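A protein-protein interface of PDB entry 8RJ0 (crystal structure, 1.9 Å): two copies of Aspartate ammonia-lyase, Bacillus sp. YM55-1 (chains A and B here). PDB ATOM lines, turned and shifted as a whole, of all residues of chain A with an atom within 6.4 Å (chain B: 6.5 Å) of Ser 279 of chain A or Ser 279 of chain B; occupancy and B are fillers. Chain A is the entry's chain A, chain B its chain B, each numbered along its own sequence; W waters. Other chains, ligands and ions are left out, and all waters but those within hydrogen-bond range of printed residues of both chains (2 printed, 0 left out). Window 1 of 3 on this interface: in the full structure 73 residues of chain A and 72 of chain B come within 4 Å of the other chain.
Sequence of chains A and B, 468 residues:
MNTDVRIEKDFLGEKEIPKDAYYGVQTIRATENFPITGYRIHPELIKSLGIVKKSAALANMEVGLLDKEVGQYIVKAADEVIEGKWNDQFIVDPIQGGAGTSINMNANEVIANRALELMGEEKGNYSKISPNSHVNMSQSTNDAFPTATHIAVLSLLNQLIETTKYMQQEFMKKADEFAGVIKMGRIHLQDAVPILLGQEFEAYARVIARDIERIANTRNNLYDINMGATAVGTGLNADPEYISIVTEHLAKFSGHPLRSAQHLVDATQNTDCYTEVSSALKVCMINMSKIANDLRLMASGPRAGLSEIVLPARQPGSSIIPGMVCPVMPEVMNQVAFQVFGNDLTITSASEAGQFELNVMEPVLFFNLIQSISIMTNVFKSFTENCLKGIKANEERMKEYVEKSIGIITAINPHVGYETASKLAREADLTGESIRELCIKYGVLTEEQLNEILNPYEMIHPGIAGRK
NZ of Lys 282 of chain B is in hydrogen-bond range of OG of Ser 279 of chain A (3.1 Å). NZ of Lys 282 of chain A lies within hydrogen-bond range of OG of Ser 279 of chain B, at 3.0 Å. OD2 of Asp 344 of chain B is in salt-bridge range of NZ of Lys 282 of chain A, at 3.0 Å. The side-chain amino group of Lys 282 of chain B lies within salt-bridge range of the side-chain carboxylate of Asp 344 of chain A, 2.9 Å away. NZ of Lys 282 of chain B sits close to NZ of Lys 282 of chain A, 3.2 Å away.
The side-chain hydroxyl (OG) of Ser 279 of chain A is in hydrogen-bond range of the backbone carbonyl oxygen (O) of Thr 275 of chain A, at 2.7 Å. OG of Ser 278 of chain A is in hydrogen-bond range of OD1 of Asp 344 of chain A. O of Asp 344 of chain A is in hydrogen-bond range of OG1 of Thr 348 of chain A, at 2.8 Å. O of Thr 275 of chain B is in hydrogen-bond range of OG of Ser 279 of chain B, at 2.8 Å. OG of Ser 278 of chain B lies within hydrogen-bond range of OD1 of Asp 344 of chain B, 2.6 Å away. The side-chain hydroxyl of Thr 348 of chain B is in hydrogen-bond range of the backbone carbonyl oxygen of Asp 344 of chain B (2.9 Å).
Thr 275 of chain A touches Val 283 of chain B. Ser 279 of chain B touches Ser 279 of chain A. Val 283 of chain B touches Ser 279 of chain A. Lys 282 of chain A touches Thr 348 of chain B (CE to OG1, 3.6 Å). CG1 of Val 283 of chain A touches OG1 of Thr 275 of chain B, at 3.6 Å. Val 283 of chain A touches Ser 279 of chain B (CG2 to OG, 3.5 Å). OG1 of Thr 348 of chain A touches CE of Lys 282 of chain B, at 3.6 Å.
Of the printed residues of chain B, Ser 279 of chain A touches Ser 279, Lys 282 and Val 283. Cys 284 of chain A touches none of the printed residues of chain B. Of the printed residues of chain B, Asp 344 of chain A touches Lys 282 (2.9 Å). Of the printed residues of chain A, Lys 282 of chain B touches Ser 279 (3.1 Å), Lys 282 (3.2 Å), Asp 344 (2.9 Å) and Thr 348 (3.6 Å). Of the printed residues of chain A, Asp 344 of chain B touches Lys 282 (3.0 Å). The nearest residue of chain B that does not touch Ser 279 of chain A is Ala 280 of chain B (5.5 Å). The nearest residue of chain A that does not touch Ser 279 of chain B is Ala 280 of chain A (5.6 Å). The nearest printed residue of chain B that does not touch Thr 275 of chain A is Lys 282 of chain B (4.9 Å).
Of the 14 printed residues of chain A, 6 touch a printed residue of chain B. Printed residues of chain A that touch a printed residue of chain B: Thr 275, Ser 279, Lys 282, Val 283, Asp 344 and Thr 348. Of the 15 printed residues of chain B, 6 touch a printed residue of chain A. Printed residues of chain B that touch a printed residue of chain A: Thr 275, Ser 279, Lys 282, Val 283, Asp 344 and Thr 348. Hydrophobic or aromatic side chains of chain B that line the printed part of chain A: Val 283. Among the printed residues, 12 pairs touch across the chains.
Ser 279 of chain B touches its own counterpart, Ser 279 of chain A. Ser 279 of chain A touches Lys 282 of chain B, and with the chains exchanged Lys 282 of chain A touches Ser 279 of chain B. Ser 279 of chain A touches Val 283 of chain B, and with the chains exchanged Val 283 of chain A touches Ser 279 of chain B. Lys 282 of chain A touches its own counterpart, Lys 282 of chain B. Positions printed for both chains: 274, 275, 276, 277, 278, 279, 280, 281, 282, 283, 284, 344, 348 and 369. Of the 12 pairs that touch across the chains among the printed residues, 12 have their exchanged pair printed and touching as well.
Water W1 lies within hydrogen-bond range of OD1 of Asp 344 of chain A, OG1 of Thr 348 of chain A and NZ of Lys 282 of chain B. Water W2 lies within hydrogen-bond range of the side-chain carboxylate of Asp 344 of chain B (2.9 Å), the side-chain hydroxyl of Thr 348 of chain B (2.9 Å) and the side-chain amino group of Lys 282 of chain A (3.3 Å).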
ATOM      1  N   TYR A 274     -30.254 -20.349 -27.122  1.00  0.00           N
ATOM      2  CA  TYR A 274     -29.474 -21.545 -27.421  1.00  0.00           C
ATOM      3  C   TYR A 274     -28.377 -21.790 -26.366  1.00  0.00           C
ATOM      4  O   TYR A 274     -28.107 -22.924 -26.003  1.00  0.00           O
ATOM      5  CB  TYR A 274     -28.852 -21.535 -28.796  1.00  0.00           C
ATOM      6  CG  TYR A 274     -29.851 -21.184 -29.868  1.00  0.00           C
ATOM      7  CD1 TYR A 274     -30.926 -22.019 -30.179  1.00  0.00           C
ATOM      8  CD2 TYR A 274     -29.743 -19.976 -30.540  1.00  0.00           C
ATOM      9  CE1 TYR A 274     -31.847 -21.648 -31.156  1.00  0.00           C
ATOM     10  CE2 TYR A 274     -30.663 -19.604 -31.513  1.00  0.00           C
ATOM     11  CZ  TYR A 274     -31.698 -20.454 -31.818  1.00  0.00           C
ATOM     12  OH  TYR A 274     -32.509 -20.053 -32.800  1.00  0.00           O
ATOM     13  N   THR A 275     -27.733 -20.747 -25.880  1.00  0.00           N
ATOM     14  CA  THR A 275     -26.680 -20.935 -24.904  1.00  0.00           C
ATOM     15  C   THR A 275     -27.285 -21.337 -23.561  1.00  0.00           C
ATOM     16  O   THR A 275     -26.639 -22.005 -22.770  1.00  0.00           O
ATOM     17  CB  THR A 275     -25.844 -19.650 -24.820  1.00  0.00           C
ATOM     18  OG1 THR A 275     -26.692 -18.538 -24.543  1.00  0.00           O
ATOM     19  CG2 THR A 275     -25.227 -19.351 -26.165  1.00  0.00           C
ATOM     20  N   GLU A 276     -28.488 -20.858 -23.271  1.00  0.00           N
ATOM     21  CA  GLU A 276     -29.211 -21.251 -22.073  1.00  0.00           C
ATOM     22  C   GLU A 276     -29.436 -22.760 -22.089  1.00  0.00           C
ATOM     23  O   GLU A 276     -29.175 -23.442 -21.119  1.00  0.00           O
ATOM     24  CB  GLU A 276     -30.490 -20.453 -22.001  1.00  0.00           C
ATOM     25  CG  GLU A 276     -31.376 -20.821 -20.816  1.00  0.00           C
ATOM     26  CD  GLU A 276     -32.713 -20.065 -20.807  1.00  0.00           C
ATOM     27  OE1 GLU A 276     -33.635 -20.483 -20.085  1.00  0.00           O
ATOM     28  OE2 GLU A 276     -32.816 -19.019 -21.454  1.00  0.00           O
ATOM     29  N   VAL A 277     -29.860 -23.296 -23.220  1.00  0.00           N
ATOM     30  CA  VAL A 277     -30.027 -24.724 -23.337  1.00  0.00           C
ATOM     31  C   VAL A 277     -28.681 -25.413 -23.144  1.00  0.00           C
ATOM     32  O   VAL A 277     -28.611 -26.305 -22.309  1.00  0.00           O
ATOM     33  CB  VAL A 277     -30.633 -25.162 -24.682  1.00  0.00           C
ATOM     34  CG1 VAL A 277     -30.768 -26.671 -24.727  1.00  0.00           C
ATOM     35  CG2 VAL A 277     -32.004 -24.504 -24.848  1.00  0.00           C
ATOM     36  N   SER A 278     -27.636 -24.980 -23.881  1.00  0.00           N
ATOM     37  CA  SER A 278     -26.361 -25.679 -23.804  1.00  0.00           C
ATOM     38  C   SER A 278     -25.855 -25.696 -22.359  1.00  0.00           C
ATOM     39  O   SER A 278     -25.331 -26.699 -21.896  1.00  0.00           O
ATOM     40  CB  SER A 278     -25.306 -25.063 -24.743  1.00  0.00           C
ATOM     41  OG  SER A 278     -24.099 -25.802 -24.659  1.00  0.00           O
ATOM     42  N   SER A 279     -26.001 -24.562 -21.662  1.00  0.00           N
ATOM     43  CA  SER A 279     -25.619 -24.455 -20.262  1.00  0.00           C
ATOM     44  C   SER A 279     -26.283 -25.494 -19.388  1.00  0.00           C
ATOM     45  O   SER A 279     -25.611 -26.083 -18.557  1.00  0.00           O
ATOM     46  CB  SER A 279     -25.954 -23.060 -19.671  1.00  0.00           C
ATOM     47  OG  SER A 279     -25.208 -22.140 -20.444  1.00  0.00           O
ATOM     48  N   ALA A 280     -27.594 -25.728 -19.574  1.00  0.00           N
ATOM     49  CA  ALA A 280     -28.266 -26.685 -18.702  1.00  0.00           C
ATOM     50  C   ALA A 280     -27.779 -28.118 -19.031  1.00  0.00           C
ATOM     51  O   ALA A 280     -27.620 -28.953 -18.147  1.00  0.00           O
ATOM     52  CB  ALA A 280     -29.718 -26.570 -18.834  1.00  0.00           C
ATOM     53  N   LEU A 281     -27.455 -28.360 -20.302  1.00  0.00           N
ATOM     54  CA  LEU A 281     -26.931 -29.657 -20.718  1.00  0.00           C
ATOM     55  C   LEU A 281     -25.544 -29.891 -20.114  1.00  0.00           C
ATOM     56  O   LEU A 281     -25.304 -30.960 -19.572  1.00  0.00           O
ATOM     57  CB  LEU A 281     -26.880 -29.747 -22.234  1.00  0.00           C
ATOM     58  CG  LEU A 281     -28.231 -29.628 -22.920  1.00  0.00           C
ATOM     59  CD1 LEU A 281     -28.002 -29.627 -24.388  1.00  0.00           C
ATOM     60  CD2 LEU A 281     -29.291 -30.639 -22.490  1.00  0.00           C
ATOM     61  N   LYS A 282     -24.696 -28.848 -20.121  1.00  0.00           N
ATOM     62  CA  LYS A 282     -23.359 -28.947 -19.551  1.00  0.00           C
ATOM     63  C   LYS A 282     -23.487 -29.257 -18.070  1.00  0.00           C
ATOM     64  O   LYS A 282     -22.837 -30.148 -17.595  1.00  0.00           O
ATOM     65  CB  LYS A 282     -22.574 -27.669 -19.815  1.00  0.00           C
ATOM     66  CG  LYS A 282     -21.139 -27.564 -19.210  1.00  0.00           C
ATOM     67  CD  LYS A 282     -20.670 -26.090 -19.137  1.00  0.00           C
ATOM     68  CE  LYS A 282     -21.209 -25.221 -17.939  1.00  0.00           C
ATOM     69  NZ  LYS A 282     -21.328 -23.719 -18.033  1.00  0.00           N
ATOM     70  N   VAL A 283     -24.274 -28.461 -17.332  1.00  0.00           N
ATOM     71  CA  VAL A 283     -24.435 -28.671 -15.901  1.00  0.00           C
ATOM     72  C   VAL A 283     -24.893 -30.110 -15.629  1.00  0.00           C
ATOM     73  O   VAL A 283     -24.339 -30.800 -14.810  1.00  0.00           O
ATOM     74  CB  VAL A 283     -25.429 -27.665 -15.308  1.00  0.00           C
ATOM     75  CG1 VAL A 283     -25.815 -28.107 -13.902  1.00  0.00           C
ATOM     76  CG2 VAL A 283     -24.821 -26.235 -15.282  1.00  0.00           C
ATOM     77  N   CYS A 284     -25.871 -30.589 -16.382  1.00  0.00           N
ATOM     78  CA  CYS A 284     -26.318 -31.965 -16.202  1.00  0.00           C
ATOM     79  C   CYS A 284     -25.137 -32.932 -16.362  1.00  0.00           C
ATOM     80  O   CYS A 284     -24.944 -33.840 -15.557  1.00  0.00           O
ATOM     81  CB  CYS A 284     -27.457 -32.236 -17.197  1.00  0.00           C
ATOM     82  SG  CYS A 284     -27.972 -33.975 -17.179  1.00  0.00           S
ATOM     83  N   ASP A 344     -20.213 -27.100 -25.707  1.00  0.00           N
ATOM     84  CA  ASP A 344     -20.731 -25.901 -25.058  1.00  0.00           C
ATOM     85  C   ASP A 344     -19.773 -24.724 -25.273  1.00  0.00           C
ATOM     86  O   ASP A 344     -20.178 -23.579 -25.333  1.00  0.00           O
ATOM     87  CB  ASP A 344     -20.966 -26.138 -23.557  1.00  0.00           C
ATOM     88  CG  ASP A 344     -21.426 -24.882 -22.814  1.00  0.00           C
ATOM     89  OD1 ASP A 344     -22.583 -24.507 -22.980  1.00  0.00           O
ATOM     90  OD2 ASP A 344     -20.571 -24.269 -22.140  1.00  0.00           O
ATOM     91  N   THR A 348     -20.669 -21.327 -27.101  1.00  0.00           N
ATOM     92  CA  THR A 348     -20.365 -20.048 -26.499  1.00  0.00           C
ATOM     93  C   THR A 348     -19.678 -19.123 -27.491  1.00  0.00           C
ATOM     94  O   THR A 348     -20.050 -17.944 -27.670  1.00  0.00           O
ATOM     95  CB  THR A 348     -19.498 -20.342 -25.286  1.00  0.00           C
ATOM     96  OG1 THR A 348     -20.297 -20.997 -24.306  1.00  0.00           O
ATOM     97  CG2 THR A 348     -18.946 -19.059 -24.705  1.00  0.00           C
ATOM     98  N   LEU A 369     -25.466 -28.088 -30.594  1.00  0.00           N
ATOM     99  CA  LEU A 369     -26.499 -28.169 -29.594  1.00  0.00           C
ATOM    100  C   LEU A 369     -27.306 -29.439 -29.816  1.00  0.00           C
ATOM    101  O   LEU A 369     -27.648 -30.130 -28.893  1.00  0.00           O
ATOM    102  CB  LEU A 369     -27.346 -26.913 -29.650  1.00  0.00           C
ATOM    103  CG  LEU A 369     -28.497 -26.840 -28.628  1.00  0.00           C
ATOM    104  CD1 LEU A 369     -27.947 -26.705 -27.247  1.00  0.00           C
ATOM    105  CD2 LEU A 369     -29.385 -25.671 -28.953  1.00  0.00           C
ATOM    106  N   THR B 218     -31.363 -18.466 -10.665  1.00  0.00           N
ATOM    107  CA  THR B 218     -30.334 -19.328 -10.105  1.00  0.00           C
ATOM    108  C   THR B 218     -30.217 -19.204  -8.596  1.00  0.00           C
ATOM    109  O   THR B 218     -29.609 -20.048  -7.945  1.00  0.00           O
ATOM    110  CB  THR B 218     -28.959 -19.117 -10.751  1.00  0.00           C
ATOM    111  OG1 THR B 218     -28.400 -17.854 -10.386  1.00  0.00           O
ATOM    112  CG2 THR B 218     -29.070 -19.301 -12.232  1.00  0.00           C
ATOM    113  N   TYR B 274     -23.857 -24.231  -7.922  1.00  0.00           N
ATOM    114  CA  TYR B 274     -22.839 -23.261  -8.277  1.00  0.00           C
ATOM    115  C   TYR B 274     -22.623 -23.185  -9.773  1.00  0.00           C
ATOM    116  O   TYR B 274     -22.391 -22.096 -10.273  1.00  0.00           O
ATOM    117  CB  TYR B 274     -21.511 -23.514  -7.594  1.00  0.00           C
ATOM    118  CG  TYR B 274     -21.650 -23.731  -6.093  1.00  0.00           C
ATOM    119  CD1 TYR B 274     -22.056 -22.707  -5.244  1.00  0.00           C
ATOM    120  CD2 TYR B 274     -21.405 -24.981  -5.551  1.00  0.00           C
ATOM    121  CE1 TYR B 274     -22.144 -22.932  -3.877  1.00  0.00           C
ATOM    122  CE2 TYR B 274     -21.509 -25.222  -4.174  1.00  0.00           C
ATOM    123  CZ  TYR B 274     -21.882 -24.186  -3.344  1.00  0.00           C
ATOM    124  OH  TYR B 274     -21.922 -24.483  -2.004  1.00  0.00           O
ATOM    125  N   THR B 275     -22.633 -24.323 -10.492  1.00  0.00           N
ATOM    126  CA  THR B 275     -22.383 -24.258 -11.914  1.00  0.00           C
ATOM    127  C   THR B 275     -23.597 -23.652 -12.594  1.00  0.00           C
ATOM    128  O   THR B 275     -23.465 -23.091 -13.662  1.00  0.00           O
ATOM    129  CB  THR B 275     -22.083 -25.678 -12.408  1.00  0.00           C
ATOM    130  OG1 THR B 275     -23.113 -26.593 -11.971  1.00  0.00           O
ATOM    131  CG2 THR B 275     -20.801 -26.142 -11.745  1.00  0.00           C
ATOM    132  N   GLU B 276     -24.807 -23.845 -12.014  1.00  0.00           N
ATOM    133  CA  GLU B 276     -26.000 -23.239 -12.572  1.00  0.00           C
ATOM    134  C   GLU B 276     -25.844 -21.709 -12.523  1.00  0.00           C
ATOM    135  O   GLU B 276     -26.123 -21.001 -13.497  1.00  0.00           O
ATOM    136  CB  GLU B 276     -27.205 -23.729 -11.756  1.00  0.00           C
ATOM    137  CG  GLU B 276     -28.530 -23.061 -12.072  1.00  0.00           C
ATOM    138  CD  GLU B 276     -29.682 -23.551 -11.168  1.00  0.00           C
ATOM    139  OE1 GLU B 276     -30.705 -22.820 -11.184  1.00  0.00           O
ATOM    140  OE2 GLU B 276     -29.614 -24.610 -10.481  1.00  0.00           O
ATOM    141  N   VAL B 277     -25.337 -21.178 -11.411  1.00  0.00           N
ATOM    142  CA  VAL B 277     -25.090 -19.740 -11.368  1.00  0.00           C
ATOM    143  C   VAL B 277     -24.038 -19.355 -12.415  1.00  0.00           C
ATOM    144  O   VAL B 277     -24.254 -18.393 -13.144  1.00  0.00           O
ATOM    145  CB  VAL B 277     -24.605 -19.210 -10.021  1.00  0.00           C
ATOM    146  CG1 VAL B 277     -24.373 -17.720 -10.097  1.00  0.00           C
ATOM    147  CG2 VAL B 277     -25.668 -19.475  -8.969  1.00  0.00           C
ATOM    148  N   SER B 278     -22.891 -20.066 -12.430  1.00  0.00           N
ATOM    149  CA  SER B 278     -21.803 -19.668 -13.336  1.00  0.00           C
ATOM    150  C   SER B 278     -22.324 -19.639 -14.779  1.00  0.00           C
ATOM    151  O   SER B 278     -21.996 -18.744 -15.559  1.00  0.00           O
ATOM    152  CB  SER B 278     -20.578 -20.543 -13.141  1.00  0.00           C
ATOM    153  OG  SER B 278     -19.579 -20.212 -14.090  1.00  0.00           O
ATOM    154  N   SER B 279     -23.150 -20.646 -15.140  1.00  0.00           N
ATOM    155  CA  SER B 279     -23.733 -20.721 -16.466  1.00  0.00           C
ATOM    156  C   SER B 279     -24.569 -19.508 -16.856  1.00  0.00           C
ATOM    157  O   SER B 279     -24.407 -19.008 -17.966  1.00  0.00           O
ATOM    158  CB  SER B 279     -24.647 -21.965 -16.563  1.00  0.00           C
ATOM    159  OG  SER B 279     -23.780 -23.088 -16.422  1.00  0.00           O
ATOM    160  N   ALA B 280     -25.394 -19.000 -15.944  1.00  0.00           N
ATOM    161  CA  ALA B 280     -26.231 -17.855 -16.226  1.00  0.00           C
ATOM    162  C   ALA B 280     -25.371 -16.599 -16.357  1.00  0.00           C
ATOM    163  O   ALA B 280     -25.630 -15.751 -17.232  1.00  0.00           O
ATOM    164  CB  ALA B 280     -27.277 -17.721 -15.144  1.00  0.00           C
ATOM    165  N   LEU B 281     -24.274 -16.533 -15.572  1.00  0.00           N
ATOM    166  CA  LEU B 281     -23.329 -15.421 -15.680  1.00  0.00           C
ATOM    167  C   LEU B 281     -22.613 -15.444 -17.033  1.00  0.00           C
ATOM    168  O   LEU B 281     -22.529 -14.426 -17.689  1.00  0.00           O
ATOM    169  CB  LEU B 281     -22.323 -15.460 -14.533  1.00  0.00           C
ATOM    170  CG  LEU B 281     -22.914 -15.431 -13.125  1.00  0.00           C
ATOM    171  CD1 LEU B 281     -21.724 -15.526 -12.148  1.00  0.00           C
ATOM    172  CD2 LEU B 281     -23.771 -14.177 -12.902  1.00  0.00           C
ATOM    173  N   LYS B 282     -22.234 -16.644 -17.506  1.00  0.00           N
ATOM    174  CA  LYS B 282     -21.554 -16.796 -18.770  1.00  0.00           C
ATOM    175  C   LYS B 282     -22.498 -16.343 -19.868  1.00  0.00           C
ATOM    176  O   LYS B 282     -22.094 -15.590 -20.746  1.00  0.00           O
ATOM    177  CB  LYS B 282     -21.086 -18.244 -18.961  1.00  0.00           C
ATOM    178  CG  LYS B 282     -20.391 -18.622 -20.324  1.00  0.00           C
ATOM    179  CD  LYS B 282     -20.307 -20.185 -20.560  1.00  0.00           C
ATOM    180  CE  LYS B 282     -21.674 -20.842 -20.993  1.00  0.00           C
ATOM    181  NZ  LYS B 282     -22.165 -22.260 -20.750  1.00  0.00           N
ATOM    182  N   VAL B 283     -23.711 -16.889 -19.891  1.00  0.00           N
ATOM    183  CA  VAL B 283     -24.682 -16.507 -20.917  1.00  0.00           C
ATOM    184  C   VAL B 283     -24.864 -14.988 -20.968  1.00  0.00           C
ATOM    185  O   VAL B 283     -24.809 -14.350 -22.020  1.00  0.00           O
ATOM    186  CB  VAL B 283     -26.056 -17.190 -20.708  1.00  0.00           C
ATOM    187  CG1 VAL B 283     -27.102 -16.603 -21.636  1.00  0.00           C
ATOM    188  CG2 VAL B 283     -25.963 -18.692 -20.944  1.00  0.00           C
ATOM    189  N   CYS B 284     -25.038 -14.370 -19.815  1.00  0.00           N
ATOM    190  CA  CYS B 284     -25.154 -12.931 -19.772  1.00  0.00           C
ATOM    191  C   CYS B 284     -23.944 -12.238 -20.441  1.00  0.00           C
ATOM    192  O   CYS B 284     -24.098 -11.344 -21.264  1.00  0.00           O
ATOM    193  CB  CYS B 284     -25.294 -12.474 -18.325  1.00  0.00           C
ATOM    194  SG  CYS B 284     -25.392 -10.676 -18.144  1.00  0.00           S
ATOM    195  N   ASP B 344     -15.822 -19.741 -15.799  1.00  0.00           N
ATOM    196  CA  ASP B 344     -16.831 -20.799 -15.881  1.00  0.00           C
ATOM    197  C   ASP B 344     -16.217 -22.164 -16.235  1.00  0.00           C
ATOM    198  O   ASP B 344     -16.714 -23.202 -15.832  1.00  0.00           O
ATOM    199  CB  ASP B 344     -17.867 -20.416 -16.923  1.00  0.00           C
ATOM    200  CG  ASP B 344     -18.951 -21.476 -17.143  1.00  0.00           C
ATOM    201  OD1 ASP B 344     -19.814 -21.670 -16.207  1.00  0.00           O
ATOM    202  OD2 ASP B 344     -18.786 -22.187 -18.120  1.00  0.00           O
ATOM    203  N   THR B 348     -16.539 -25.413 -13.994  1.00  0.00           N
ATOM    204  CA  THR B 348     -16.954 -26.690 -14.571  1.00  0.00           C
ATOM    205  C   THR B 348     -16.013 -27.808 -14.153  1.00  0.00           C
ATOM    206  O   THR B 348     -16.410 -28.865 -13.666  1.00  0.00           O
ATOM    207  CB  THR B 348     -16.972 -26.540 -16.089  1.00  0.00           C
ATOM    208  OG1 THR B 348     -18.030 -25.691 -16.394  1.00  0.00           O
ATOM    209  CG2 THR B 348     -17.290 -27.851 -16.776  1.00  0.00           C
ATOM    210  N   LEU B 369     -16.387 -18.015  -8.831  1.00  0.00           N
ATOM    211  CA  LEU B 369     -17.770 -17.656  -8.981  1.00  0.00           C
ATOM    212  C   LEU B 369     -17.986 -16.243  -8.384  1.00  0.00           C
ATOM    213  O   LEU B 369     -18.644 -15.421  -8.955  1.00  0.00           O
ATOM    214  CB  LEU B 369     -18.618 -18.672  -8.241  1.00  0.00           C
ATOM    215  CG  LEU B 369     -20.118 -18.463  -8.289  1.00  0.00           C
ATOM    216  CD1 LEU B 369     -20.679 -18.555  -9.692  1.00  0.00           C
ATOM    217  CD2 LEU B 369     -20.780 -19.438  -7.394  1.00  0.00           C
HETATM  218  O   HOH W   1     -22.945 -21.904 -23.898  1.00  0.00           O
HETATM  219  O   HOH W   2     -20.149 -24.251 -14.949  1.00  0.00           O
